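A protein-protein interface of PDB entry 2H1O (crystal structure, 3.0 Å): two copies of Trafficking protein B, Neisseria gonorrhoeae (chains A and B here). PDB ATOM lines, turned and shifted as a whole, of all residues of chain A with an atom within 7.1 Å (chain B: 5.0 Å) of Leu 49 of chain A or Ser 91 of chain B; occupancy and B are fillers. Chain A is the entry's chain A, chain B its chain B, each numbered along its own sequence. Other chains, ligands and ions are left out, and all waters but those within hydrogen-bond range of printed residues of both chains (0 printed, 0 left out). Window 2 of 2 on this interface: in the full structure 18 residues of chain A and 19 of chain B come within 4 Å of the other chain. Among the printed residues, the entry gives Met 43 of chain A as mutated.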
ATOM      1  N   MET A  43     -12.075  15.312   5.616  1.00  0.00           N
ATOM      2  CA  MET A  43     -11.492  14.744   4.411  1.00  0.00           C
ATOM      3  C   MET A  43     -11.205  15.861   3.426  1.00  0.00           C
ATOM      4  O   MET A  43     -10.083  16.008   2.940  1.00  0.00           O
ATOM      5  CB  MET A  43     -12.461  13.771   3.755  1.00  0.00           C
ATOM      6  CG  MET A  43     -12.479  12.377   4.328  1.00  0.00           C
ATOM      7  SD  MET A  43     -13.921  11.472   3.658  1.00  0.00           S
ATOM      8  CE  MET A  43     -13.291  10.880   2.058  1.00  0.00           C
ATOM      9  N   ARG A  44     -12.235  16.642   3.129  1.00  0.00           N
ATOM     10  CA  ARG A  44     -12.116  17.741   2.185  1.00  0.00           C
ATOM     11  C   ARG A  44     -10.990  18.723   2.531  1.00  0.00           C
ATOM     12  O   ARG A  44     -10.325  19.246   1.633  1.00  0.00           O
ATOM     13  CB  ARG A  44     -13.456  18.464   2.078  1.00  0.00           C
ATOM     14  CG  ARG A  44     -14.541  17.670   1.372  1.00  0.00           C
ATOM     15  CD  ARG A  44     -14.806  18.276   0.031  1.00  0.00           C
ATOM     16  NE  ARG A  44     -16.061  17.813  -0.544  1.00  0.00           N
ATOM     17  CZ  ARG A  44     -17.255  17.983   0.014  1.00  0.00           C
ATOM     18  NH1 ARG A  44     -17.373  18.609   1.176  1.00  0.00           N
ATOM     19  NH2 ARG A  44     -18.338  17.538  -0.600  1.00  0.00           N
ATOM     20  N   LEU A  45     -10.772  18.965   3.822  1.00  0.00           N
ATOM     21  CA  LEU A  45      -9.705  19.870   4.261  1.00  0.00           C
ATOM     22  C   LEU A  45      -8.355  19.166   4.197  1.00  0.00           C
ATOM     23  O   LEU A  45      -7.338  19.771   3.864  1.00  0.00           O
ATOM     24  CB  LEU A  45      -9.944  20.349   5.701  1.00  0.00           C
ATOM     25  CG  LEU A  45      -8.790  21.097   6.383  1.00  0.00           C
ATOM     26  CD1 LEU A  45      -8.394  22.270   5.538  1.00  0.00           C
ATOM     27  CD2 LEU A  45      -9.197  21.567   7.761  1.00  0.00           C
ATOM     28  N   GLY A  46      -8.347  17.883   4.525  1.00  0.00           N
ATOM     29  CA  GLY A  46      -7.102  17.141   4.492  1.00  0.00           C
ATOM     30  C   GLY A  46      -6.500  17.123   3.104  1.00  0.00           C
ATOM     31  O   GLY A  46      -5.283  17.011   2.937  1.00  0.00           O
ATOM     32  N   VAL A  47      -7.365  17.212   2.101  1.00  0.00           N
ATOM     33  CA  VAL A  47      -6.917  17.214   0.723  1.00  0.00           C
ATOM     34  C   VAL A  47      -6.412  18.616   0.414  1.00  0.00           C
ATOM     35  O   VAL A  47      -5.269  18.798  -0.004  1.00  0.00           O
ATOM     36  CB  VAL A  47      -8.074  16.839  -0.230  1.00  0.00           C
ATOM     37  CG1 VAL A  47      -7.672  17.075  -1.681  1.00  0.00           C
ATOM     38  CG2 VAL A  47      -8.442  15.387  -0.027  1.00  0.00           C
ATOM     39  N   ALA A  48      -7.267  19.604   0.651  1.00  0.00           N
ATOM     40  CA  ALA A  48      -6.928  20.999   0.409  1.00  0.00           C
ATOM     41  C   ALA A  48      -5.561  21.432   0.959  1.00  0.00           C
ATOM     42  O   ALA A  48      -4.902  22.299   0.378  1.00  0.00           O
ATOM     43  CB  ALA A  48      -8.007  21.874   0.994  1.00  0.00           C
ATOM     44  N   LEU A  49      -5.136  20.831   2.068  1.00  0.00           N
ATOM     45  CA  LEU A  49      -3.869  21.196   2.691  1.00  0.00           C
ATOM     46  C   LEU A  49      -2.595  20.643   2.060  1.00  0.00           C
ATOM     47  O   LEU A  49      -1.501  20.992   2.494  1.00  0.00           O
ATOM     48  CB  LEU A  49      -3.878  20.819   4.173  1.00  0.00           C
ATOM     49  CG  LEU A  49      -4.777  21.606   5.126  1.00  0.00           C
ATOM     50  CD1 LEU A  49      -4.671  21.018   6.512  1.00  0.00           C
ATOM     51  CD2 LEU A  49      -4.370  23.059   5.158  1.00  0.00           C
ATOM     52  N   LEU A  50      -2.718  19.791   1.050  1.00  0.00           N
ATOM     53  CA  LEU A  50      -1.540  19.220   0.394  1.00  0.00           C
ATOM     54  C   LEU A  50      -0.863  20.245  -0.514  1.00  0.00           C
ATOM     55  O   LEU A  50      -1.546  21.112  -1.074  1.00  0.00           O
ATOM     56  CB  LEU A  50      -1.944  18.012  -0.459  1.00  0.00           C
ATOM     57  CG  LEU A  50      -2.285  16.687   0.223  1.00  0.00           C
ATOM     58  CD1 LEU A  50      -2.779  15.705  -0.818  1.00  0.00           C
ATOM     59  CD2 LEU A  50      -1.059  16.141   0.945  1.00  0.00           C
ATOM     60  N   LEU A  51       0.464  20.152  -0.670  1.00  0.00           N
ATOM     61  CA  LEU A  51       1.188  21.072  -1.552  1.00  0.00           C
ATOM     62  C   LEU A  51       0.667  20.902  -2.979  1.00  0.00           C
ATOM     63  O   LEU A  51       0.438  19.784  -3.450  1.00  0.00           O
ATOM     64  CB  LEU A  51       2.696  20.793  -1.550  1.00  0.00           C
ATOM     65  CG  LEU A  51       3.511  20.931  -0.260  1.00  0.00           C
ATOM     66  CD1 LEU A  51       4.995  20.933  -0.586  1.00  0.00           C
ATOM     67  CD2 LEU A  51       3.138  22.215   0.448  1.00  0.00           C
ATOM     68  N   ASN A  52       0.488  22.016  -3.671  1.00  0.00           N
ATOM     69  CA  ASN A  52      -0.019  21.980  -5.032  1.00  0.00           C
ATOM     70  C   ASN A  52       0.847  21.164  -5.975  1.00  0.00           C
ATOM     71  O   ASN A  52       2.031  21.433  -6.153  1.00  0.00           O
ATOM     72  CB  ASN A  52      -0.190  23.406  -5.545  1.00  0.00           C
ATOM     73  CG  ASN A  52      -1.396  24.092  -4.932  1.00  0.00           C
ATOM     74  OD1 ASN A  52      -2.519  23.939  -5.417  1.00  0.00           O
ATOM     75  ND2 ASN A  52      -1.178  24.831  -3.845  1.00  0.00           N
ATOM     76  N   LYS A  56      -2.323  15.980  -5.576  1.00  0.00           N
ATOM     77  CA  LYS A  56      -3.457  16.661  -4.973  1.00  0.00           C
ATOM     78  C   LYS A  56      -4.617  16.896  -5.928  1.00  0.00           C
ATOM     79  O   LYS A  56      -5.766  16.910  -5.504  1.00  0.00           O
ATOM     80  CB  LYS A  56      -3.007  17.986  -4.364  1.00  0.00           C
ATOM     81  CG  LYS A  56      -4.140  18.880  -3.954  1.00  0.00           C
ATOM     82  CD  LYS A  56      -3.617  20.113  -3.272  1.00  0.00           C
ATOM     83  CE  LYS A  56      -4.696  21.165  -3.169  1.00  0.00           C
ATOM     84  NZ  LYS A  56      -4.223  22.343  -2.398  1.00  0.00           N
ATOM     85  N   TYR B  86     -16.229  24.973   4.433  1.00  0.00           N
ATOM     86  CA  TYR B  86     -15.312  24.847   5.555  1.00  0.00           C
ATOM     87  C   TYR B  86     -13.905  24.551   5.026  1.00  0.00           C
ATOM     88  O   TYR B  86     -12.963  25.288   5.303  1.00  0.00           O
ATOM     89  CB  TYR B  86     -15.776  23.702   6.447  1.00  0.00           C
ATOM     90  CG  TYR B  86     -14.833  23.333   7.554  1.00  0.00           C
ATOM     91  CD1 TYR B  86     -14.886  23.985   8.765  1.00  0.00           C
ATOM     92  CD2 TYR B  86     -13.894  22.323   7.390  1.00  0.00           C
ATOM     93  CE1 TYR B  86     -14.025  23.644   9.804  1.00  0.00           C
ATOM     94  CE2 TYR B  86     -13.028  21.973   8.414  1.00  0.00           C
ATOM     95  CZ  TYR B  86     -13.101  22.639   9.624  1.00  0.00           C
ATOM     96  OH  TYR B  86     -12.269  22.320  10.674  1.00  0.00           O
ATOM     97  N   ALA B  87     -13.771  23.481   4.250  1.00  0.00           N
ATOM     98  CA  ALA B  87     -12.479  23.087   3.698  1.00  0.00           C
ATOM     99  C   ALA B  87     -11.761  24.218   3.001  1.00  0.00           C
ATOM    100  O   ALA B  87     -10.565  24.409   3.215  1.00  0.00           O
ATOM    101  CB  ALA B  87     -12.645  21.927   2.722  1.00  0.00           C
ATOM    102  N   GLN B  88     -12.476  24.949   2.147  1.00  0.00           N
ATOM    103  CA  GLN B  88     -11.888  26.068   1.419  1.00  0.00           C
ATOM    104  C   GLN B  88     -11.412  27.125   2.421  1.00  0.00           C
ATOM    105  O   GLN B  88     -10.211  27.403   2.528  1.00  0.00           O
ATOM    106  CB  GLN B  88     -12.923  26.655   0.451  1.00  0.00           C
ATOM    107  CG  GLN B  88     -12.445  27.823  -0.445  1.00  0.00           C
ATOM    108  CD  GLN B  88     -12.460  29.198   0.252  1.00  0.00           C
ATOM    109  OE1 GLN B  88     -13.489  29.648   0.786  1.00  0.00           O
ATOM    110  NE2 GLN B  88     -11.315  29.873   0.229  1.00  0.00           N
ATOM    111  N   ILE B  89     -12.351  27.701   3.162  1.00  0.00           N
ATOM    112  CA  ILE B  89     -12.007  28.706   4.151  1.00  0.00           C
ATOM    113  C   ILE B  89     -10.767  28.297   4.937  1.00  0.00           C
ATOM    114  O   ILE B  89      -9.739  28.960   4.855  1.00  0.00           O
ATOM    115  CB  ILE B  89     -13.147  28.928   5.148  1.00  0.00           C
ATOM    116  CG1 ILE B  89     -14.345  29.559   4.436  1.00  0.00           C
ATOM    117  CG2 ILE B  89     -12.667  29.776   6.282  1.00  0.00           C
ATOM    118  CD1 ILE B  89     -15.590  29.669   5.284  1.00  0.00           C
ATOM    119  N   ARG B  90     -10.837  27.198   5.681  1.00  0.00           N
ATOM    120  CA  ARG B  90      -9.685  26.806   6.482  1.00  0.00           C
ATOM    121  C   ARG B  90      -8.417  26.500   5.709  1.00  0.00           C
ATOM    122  O   ARG B  90      -7.355  27.003   6.050  1.00  0.00           O
ATOM    123  CB  ARG B  90     -10.024  25.637   7.401  1.00  0.00           C
ATOM    124  CG  ARG B  90     -10.812  26.040   8.614  1.00  0.00           C
ATOM    125  CD  ARG B  90     -10.769  24.953   9.650  1.00  0.00           C
ATOM    126  NE  ARG B  90      -9.485  24.919  10.345  1.00  0.00           N
ATOM    127  CZ  ARG B  90      -9.090  23.930  11.142  1.00  0.00           C
ATOM    128  NH1 ARG B  90      -9.883  22.883  11.345  1.00  0.00           N
ATOM    129  NH2 ARG B  90      -7.903  23.982  11.740  1.00  0.00           N
ATOM    130  N   SER B  91      -8.501  25.684   4.672  1.00  0.00           N
ATOM    131  CA  SER B  91      -7.294  25.380   3.929  1.00  0.00           C
ATOM    132  C   SER B  91      -6.696  26.686   3.427  1.00  0.00           C
ATOM    133  O   SER B  91      -5.499  26.904   3.514  1.00  0.00           O
ATOM    134  CB  SER B  91      -7.598  24.477   2.748  1.00  0.00           C
ATOM    135  OG  SER B  91      -8.228  25.224   1.735  1.00  0.00           O
ATOM    136  N   TYR B  92      -7.527  27.577   2.916  1.00  0.00           N
ATOM    137  CA  TYR B  92      -6.994  28.838   2.426  1.00  0.00           C
ATOM    138  C   TYR B  92      -6.169  29.597   3.486  1.00  0.00           C
ATOM    139  O   TYR B  92      -4.956  29.738   3.361  1.00  0.00           O
ATOM    140  CB  TYR B  92      -8.119  29.737   1.933  1.00  0.00           C
ATOM    141  CG  TYR B  92      -7.587  30.900   1.153  1.00  0.00           C
ATOM    142  CD1 TYR B  92      -7.309  30.778  -0.209  1.00  0.00           C
ATOM    143  CD2 TYR B  92      -7.242  32.082   1.797  1.00  0.00           C
ATOM    144  CE1 TYR B  92      -6.689  31.806  -0.913  1.00  0.00           C
ATOM    145  CE2 TYR B  92      -6.616  33.119   1.110  1.00  0.00           C
ATOM    146  CZ  TYR B  92      -6.337  32.977  -0.244  1.00  0.00           C
ATOM    147  OH  TYR B  92      -5.678  33.993  -0.908  1.00  0.00           O
ATOM    148  N   ALA B  93      -6.838  30.093   4.521  1.00  0.00           N
ATOM    149  CA  ALA B  93      -6.172  30.835   5.589  1.00  0.00           C
ATOM    150  C   ALA B  93      -4.890  30.158   6.072  1.00  0.00           C
ATOM    151  O   ALA B  93      -3.817  30.772   6.132  1.00  0.00           O
ATOM    152  CB  ALA B  93      -7.134  31.011   6.767  1.00  0.00           C
ATOM    153  N   LYS B  94      -5.023  28.889   6.438  1.00  0.00           N
ATOM    154  CA  LYS B  94      -3.908  28.113   6.938  1.00  0.00           C
ATOM    155  C   LYS B  94      -2.728  28.151   5.995  1.00  0.00           C
ATOM    156  O   LYS B  94      -1.584  28.315   6.434  1.00  0.00           O
ATOM    157  CB  LYS B  94      -4.320  26.663   7.166  1.00  0.00           C
ATOM    158  CG  LYS B  94      -4.753  26.313   8.584  1.00  0.00           C
ATOM    159  CD  LYS B  94      -5.256  24.867   8.604  1.00  0.00           C
ATOM    160  CE  LYS B  94      -5.437  24.324  10.010  1.00  0.00           C
ATOM    161  NZ  LYS B  94      -4.140  24.208  10.748  1.00  0.00           N
ATOM    162  N   THR B  95      -2.972  28.002   4.703  1.00  0.00           N
ATOM    163  CA  THR B  95      -1.834  28.027   3.811  1.00  0.00           C
ATOM    164  C   THR B  95      -1.351  29.436   3.496  1.00  0.00           C
ATOM    165  O   THR B  95      -0.498  29.614   2.640  1.00  0.00           O
ATOM    166  CB  THR B  95      -2.089  27.254   2.490  1.00  0.00           C
ATOM    167  OG1 THR B  95      -3.007  27.975   1.664  1.00  0.00           O
ATOM    168  CG2 THR B  95      -2.624  25.874   2.779  1.00  0.00           C
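The backbone carbonyl oxygen of Ala 48 of chain A lies within hydrogen-bond range of the side-chain amino group of Lys 56 of chain A (2.9 Å). The guanidinium group (NH1) of Arg 90 of chain B is in hydrogen-bond range of the side-chain hydroxyl (OH) of Tyr 86 of chain B (2.5 Å). The backbone carbonyl oxygen (O) of Ala 87 of chain B is in hydrogen-bond range of the side-chain hydroxyl (OG) of Ser 91 of chain B, 2.9 Å away. O of Gln 88 of chain B sits at hydrogen-bond distance from OG of Ser 91 of chain B (3.1 Å). O of Ser 91 of chain B lies close to OG1 of Thr 95 of chain B, at 3.3 Å.
Hydrophobic or aromatic side chains of chain A within 4 Å of the printed part of chain B: Leu 45, Ala 48 and Leu 49. Along chain A the printed residues that touch a printed residue of chain B span positions 44 to 49. Hydrophobic or aromatic side chains of chain B within 4 Å of the printed part of chain A: Tyr 86 and Ala 87. Among the printed residues, no Asp or Glu carboxylate lies within 4 Å of a Lys or Arg side-chain nitrogen of the other chain.
No position is printed for both chains. Of the 8 pairs that touch across the chains among the printed residues, none has its exchanged pair printed and touching as well.
C of Arg 44 of chain A touches CB of Ala 87 of chain B (3.6 Å). Tyr 86 of chain B touches Leu 45 of chain A. N of Leu 45 of chain A touches CB of Ala 87 of chain B (3.7 Å). CD2 of Leu 45 of chain A touches NH1 of Arg 90 of chain B (3.9 Å). Leu 45 of chain A touches Ser 91 of chain B (CD1 to N, 3.5 Å). Ala 48 of chain A touches Ser 91 of chain B. Leu 49 of chain A touches Ser 91 of chain B (CD2 to CA, 3.9 Å). CD of Lys 94 of chain B touches CD2 of Leu 49 of chain A, at 3.99 Å.
Met 43 of chain A touches none of the printed residues of chain B. Printed residues of chain B within 4 Å of Leu 45 of chain A: Tyr 86, Ala 87, Arg 90 and Ser 91. Of the printed residues of chain B, Leu 49 of chain A touches Ser 91 and Lys 94. Of the printed residues of chain A, Ala 87 of chain B touches Arg 44 and Leu 45. Ser 91 of chain B touches just these residues of chain A: Leu 45 (3.5 Å), Ala 48 (3.2 Å) and Leu 49 (3.9 Å).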
